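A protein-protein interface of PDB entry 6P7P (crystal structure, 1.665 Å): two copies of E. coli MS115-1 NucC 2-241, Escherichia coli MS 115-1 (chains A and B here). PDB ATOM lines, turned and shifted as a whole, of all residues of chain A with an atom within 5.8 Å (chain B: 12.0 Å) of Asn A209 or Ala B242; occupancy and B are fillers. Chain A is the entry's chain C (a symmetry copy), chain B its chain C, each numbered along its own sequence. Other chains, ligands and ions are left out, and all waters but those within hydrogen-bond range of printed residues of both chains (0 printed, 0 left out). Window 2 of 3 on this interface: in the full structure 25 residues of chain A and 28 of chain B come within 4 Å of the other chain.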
ATOM      1  N   SER A   9      18.017 -35.812   3.670  1.00  0.00           N
ATOM      2  CA  SER A   9      18.317 -35.602   5.078  1.00  0.00           C
ATOM      3  C   SER A   9      19.286 -36.649   5.607  1.00  0.00           C
ATOM      4  O   SER A   9      20.186 -36.332   6.395  1.00  0.00           O
ATOM      5  CB  SER A   9      17.026 -35.619   5.892  1.00  0.00           C
ATOM      6  OG  SER A   9      16.363 -34.376   5.799  1.00  0.00           O
ATOM      7  N   HIS A 207      21.564 -25.103  17.679  1.00  0.00           N
ATOM      8  CA  HIS A 207      21.780 -26.335  18.423  1.00  0.00           C
ATOM      9  C   HIS A 207      21.387 -27.540  17.586  1.00  0.00           C
ATOM     10  O   HIS A 207      20.334 -27.543  16.945  1.00  0.00           O
ATOM     11  CB  HIS A 207      20.993 -26.293  19.734  1.00  0.00           C
ATOM     12  CG  HIS A 207      21.437 -25.195  20.650  1.00  0.00           C
ATOM     13  ND1 HIS A 207      21.040 -23.885  20.484  1.00  0.00           N
ATOM     14  CD2 HIS A 207      22.290 -25.200  21.699  1.00  0.00           C
ATOM     15  CE1 HIS A 207      21.610 -23.135  21.410  1.00  0.00           C
ATOM     16  NE2 HIS A 207      22.371 -23.909  22.162  1.00  0.00           N
ATOM     17  N   GLY A 208      22.248 -28.554  17.586  1.00  0.00           N
ATOM     18  CA  GLY A 208      21.936 -29.794  16.906  1.00  0.00           C
ATOM     19  C   GLY A 208      21.767 -29.608  15.415  1.00  0.00           C
ATOM     20  O   GLY A 208      22.469 -28.816  14.772  1.00  0.00           O
ATOM     21  N   ASN A 209      20.837 -30.373  14.852  1.00  0.00           N
ATOM     22  CA  ASN A 209      20.532 -30.337  13.417  1.00  0.00           C
ATOM     23  C   ASN A 209      21.813 -30.431  12.586  1.00  0.00           C
ATOM     24  O   ASN A 209      22.115 -29.556  11.769  1.00  0.00           O
ATOM     25  CB  ASN A 209      19.739 -29.080  13.055  1.00  0.00           C
ATOM     26  CG  ASN A 209      18.381 -29.034  13.742  1.00  0.00           C
ATOM     27  OD1 ASN A 209      17.748 -30.069  13.953  1.00  0.00           O
ATOM     28  ND2 ASN A 209      17.944 -27.838  14.114  1.00  0.00           N
ATOM     29  N   LYS A 210      22.575 -31.519  12.848  1.00  0.00           N
ATOM     30  CA  LYS A 210      23.751 -31.926  12.090  1.00  0.00           C
ATOM     31  C   LYS A 210      24.827 -30.839  12.090  1.00  0.00           C
ATOM     32  O   LYS A 210      25.170 -30.289  11.034  1.00  0.00           O
ATOM     33  CB  LYS A 210      23.303 -32.308  10.677  1.00  0.00           C
ATOM     34  CG  LYS A 210      22.114 -33.289  10.669  1.00  0.00           C
ATOM     35  CD  LYS A 210      21.580 -33.550   9.266  1.00  0.00           C
ATOM     36  CE  LYS A 210      20.091 -33.924   9.254  1.00  0.00           C
ATOM     37  NZ  LYS A 210      19.681 -34.661  10.458  1.00  0.00           N
ATOM     38  N   PRO A 211      25.438 -30.583  13.251  1.00  0.00           N
ATOM     39  CA  PRO A 211      26.312 -29.399  13.402  1.00  0.00           C
ATOM     40  C   PRO A 211      27.430 -29.272  12.379  1.00  0.00           C
ATOM     41  O   PRO A 211      27.666 -28.161  11.892  1.00  0.00           O
ATOM     42  CB  PRO A 211      26.865 -29.575  14.828  1.00  0.00           C
ATOM     43  CG  PRO A 211      25.776 -30.314  15.558  1.00  0.00           C
ATOM     44  CD  PRO A 211      25.175 -31.258  14.549  1.00  0.00           C
ATOM     45  N   ALA A 214      25.933 -28.329   9.020  1.00  0.00           N
ATOM     46  CA  ALA A 214      25.431 -26.960   9.046  1.00  0.00           C
ATOM     47  C   ALA A 214      26.573 -25.956   8.989  1.00  0.00           C
ATOM     48  O   ALA A 214      26.474 -24.935   8.294  1.00  0.00           O
ATOM     49  CB  ALA A 214      24.588 -26.744  10.308  1.00  0.00           C
ATOM     50  N   SER B  66      17.640 -29.739  -4.254  1.00  0.00           N
ATOM     51  CA  SER B  66      17.317 -29.140  -2.969  1.00  0.00           C
ATOM     52  C   SER B  66      15.881 -29.373  -2.562  1.00  0.00           C
ATOM     53  O   SER B  66      15.508 -28.993  -1.446  1.00  0.00           O
ATOM     54  CB  SER B  66      17.617 -27.646  -3.022  1.00  0.00           C
ATOM     55  OG  SER B  66      16.783 -26.983  -3.956  1.00  0.00           O
ATOM     56  N   ILE B 234      23.507 -23.143  -1.481  1.00  0.00           N
ATOM     57  CA  ILE B 234      23.656 -24.286  -0.597  1.00  0.00           C
ATOM     58  C   ILE B 234      22.673 -24.197   0.569  1.00  0.00           C
ATOM     59  O   ILE B 234      22.313 -25.228   1.153  1.00  0.00           O
ATOM     60  CB  ILE B 234      25.108 -24.430  -0.107  1.00  0.00           C
ATOM     61  CG1 ILE B 234      25.320 -25.837   0.458  1.00  0.00           C
ATOM     62  CG2 ILE B 234      25.448 -23.394   0.939  1.00  0.00           C
ATOM     63  CD1 ILE B 234      25.222 -26.930  -0.580  1.00  0.00           C
ATOM     64  N   ASP B 235      22.200 -23.001   0.915  1.00  0.00           N
ATOM     65  CA  ASP B 235      21.223 -22.891   1.996  1.00  0.00           C
ATOM     66  C   ASP B 235      19.867 -23.486   1.612  1.00  0.00           C
ATOM     67  O   ASP B 235      19.091 -23.843   2.495  1.00  0.00           O
ATOM     68  CB  ASP B 235      21.081 -21.434   2.428  1.00  0.00           C
ATOM     69  CG  ASP B 235      22.320 -20.932   3.176  1.00  0.00           C
ATOM     70  OD1 ASP B 235      22.988 -21.744   3.872  1.00  0.00           O
ATOM     71  OD2 ASP B 235      22.624 -19.740   3.017  1.00  0.00           O
ATOM     72  N   ALA B 236      19.584 -23.634   0.321  1.00  0.00           N
ATOM     73  CA  ALA B 236      18.386 -24.374  -0.082  1.00  0.00           C
ATOM     74  C   ALA B 236      18.500 -25.840   0.317  1.00  0.00           C
ATOM     75  O   ALA B 236      17.512 -26.462   0.754  1.00  0.00           O
ATOM     76  CB  ALA B 236      18.172 -24.238  -1.583  1.00  0.00           C
ATOM     77  N   TYR B 237      19.690 -26.417   0.159  1.00  0.00           N
ATOM     78  CA  TYR B 237      19.925 -27.762   0.661  1.00  0.00           C
ATOM     79  C   TYR B 237      19.859 -27.795   2.179  1.00  0.00           C
ATOM     80  O   TYR B 237      19.417 -28.789   2.762  1.00  0.00           O
ATOM     81  CB  TYR B 237      21.276 -28.278   0.159  1.00  0.00           C
ATOM     82  CG  TYR B 237      21.230 -28.617  -1.305  1.00  0.00           C
ATOM     83  CD1 TYR B 237      21.449 -27.637  -2.273  1.00  0.00           C
ATOM     84  CD2 TYR B 237      20.903 -29.893  -1.731  1.00  0.00           C
ATOM     85  CE1 TYR B 237      21.367 -27.940  -3.622  1.00  0.00           C
ATOM     86  CE2 TYR B 237      20.820 -30.202  -3.071  1.00  0.00           C
ATOM     87  CZ  TYR B 237      21.067 -29.238  -4.012  1.00  0.00           C
ATOM     88  OH  TYR B 237      20.969 -29.577  -5.349  1.00  0.00           O
ATOM     89  N   GLY B 238      20.285 -26.719   2.828  1.00  0.00           N
ATOM     90  CA  GLY B 238      20.327 -26.664   4.274  1.00  0.00           C
ATOM     91  C   GLY B 238      18.976 -26.715   4.939  1.00  0.00           C
ATOM     92  O   GLY B 238      18.905 -26.942   6.149  1.00  0.00           O
ATOM     93  N   LYS B 239      17.902 -26.526   4.182  1.00  0.00           N
ATOM     94  CA  LYS B 239      16.588 -26.691   4.771  1.00  0.00           C
ATOM     95  C   LYS B 239      16.372 -28.111   5.262  1.00  0.00           C
ATOM     96  O   LYS B 239      15.520 -28.331   6.123  1.00  0.00           O
ATOM     97  CB  LYS B 239      15.531 -26.289   3.745  1.00  0.00           C
ATOM     98  CG  LYS B 239      15.562 -24.824   3.396  1.00  0.00           C
ATOM     99  CD  LYS B 239      14.569 -24.516   2.275  1.00  0.00           C
ATOM    100  CE  LYS B 239      14.498 -23.028   1.970  1.00  0.00           C
ATOM    101  NZ  LYS B 239      13.831 -22.787   0.652  1.00  0.00           N
ATOM    102  N   TRP B 240      17.130 -29.077   4.753  1.00  0.00           N
ATOM    103  CA  TRP B 240      16.977 -30.471   5.152  1.00  0.00           C
ATOM    104  C   TRP B 240      17.813 -30.865   6.366  1.00  0.00           C
ATOM    105  O   TRP B 240      17.776 -32.031   6.777  1.00  0.00           O
ATOM    106  CB  TRP B 240      17.335 -31.385   3.979  1.00  0.00           C
ATOM    107  CG  TRP B 240      16.407 -31.185   2.840  1.00  0.00           C
ATOM    108  CD1 TRP B 240      16.547 -30.288   1.824  1.00  0.00           C
ATOM    109  CD2 TRP B 240      15.175 -31.862   2.613  1.00  0.00           C
ATOM    110  NE1 TRP B 240      15.486 -30.380   0.966  1.00  0.00           N
ATOM    111  CE2 TRP B 240      14.621 -31.332   1.434  1.00  0.00           C
ATOM    112  CE3 TRP B 240      14.475 -32.861   3.296  1.00  0.00           C
ATOM    113  CZ2 TRP B 240      13.412 -31.777   0.908  1.00  0.00           C
ATOM    114  CZ3 TRP B 240      13.269 -33.302   2.771  1.00  0.00           C
ATOM    115  CH2 TRP B 240      12.752 -32.756   1.592  1.00  0.00           C
ATOM    116  N   LEU B 241      18.552 -29.928   6.958  1.00  0.00           N
ATOM    117  CA  LEU B 241      19.282 -30.236   8.182  1.00  0.00           C
ATOM    118  C   LEU B 241      18.348 -30.403   9.372  1.00  0.00           C
ATOM    119  O   LEU B 241      18.670 -31.133  10.311  1.00  0.00           O
ATOM    120  CB  LEU B 241      20.286 -29.132   8.464  1.00  0.00           C
ATOM    121  CG  LEU B 241      21.326 -28.937   7.360  1.00  0.00           C
ATOM    122  CD1 LEU B 241      22.122 -27.658   7.599  1.00  0.00           C
ATOM    123  CD2 LEU B 241      22.221 -30.134   7.304  1.00  0.00           C
ATOM    124  N   ALA B 242      17.219 -29.710   9.368  1.00  0.00           N
ATOM    125  CA  ALA B 242      16.271 -29.785  10.482  1.00  0.00           C
ATOM    126  C   ALA B 242      15.141 -30.757  10.167  1.00  0.00           C
ATOM    127  O   ALA B 242      15.392 -31.923   9.857  1.00  0.00           O
ATOM    128  CB  ALA B 242      15.711 -28.415  10.801  1.00  0.00           C
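Of the printed residues of chain B, Ser A9 touches Trp B240 (2.9 Å).
No residue of chain B comes within 4 Å of Gly A208.
Of chain B, only Trp B240 and Leu B241 come within 4 Å of Lys A210.
Ser B66 touches none of the printed residues of chain A.
Tyr B237 touches none of the printed residues of chain A.
Of the printed residues of chain A, Trp B240 touches Ser A9 and Lys A210.
Of the printed residues of chain A, Leu B241 touches Asn A209 (3.6 Å), Lys A210 (3.3 Å) and Ala A214 (3.7 Å).
Ala B242 touches just one residue of chain A: Asn A209 (3.8 Å).
The nearest residue of chain B that does not touch Asn A209 is Gly B238 (7.0 Å).
The nearest printed residue of chain A that does not touch Ala B242 is Ser A9 (4.8 Å).
The nearest printed residue of chain A that does not touch Trp B240 is Asn A209 (7.0 Å).
Hydrophobic or aromatic side chains of chain A that line the printed part of chain B: Ala A214.
Hydrophobic or aromatic side chains of chain B within 4 Å of the printed part of chain A: Trp B240 and Leu B241.
Among the printed residues, no Asp or Glu carboxylate lies within 4 Å of a Lys or Arg side-chain nitrogen of the other chain.
Among the printed residues, merely in contact across the chains: Asn A209 with Leu B241 (3.6 Å), Asn A209 with Ala B242 (3.8 Å), Lys A210 with Trp B240 (3.9 Å), Lys A210 with Leu B241 (3.3 Å) and Ala A214 with Leu B241 (3.7 Å).
No position is printed for both chains.
O of Ser B66 lies within hydrogen-bond range of NE1 of Trp B240, 2.8 Å away.
The backbone carbonyl oxygen of Trp B240 is in hydrogen-bond range of the side-chain hydroxyl of Ser A9 (2.9 Å).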
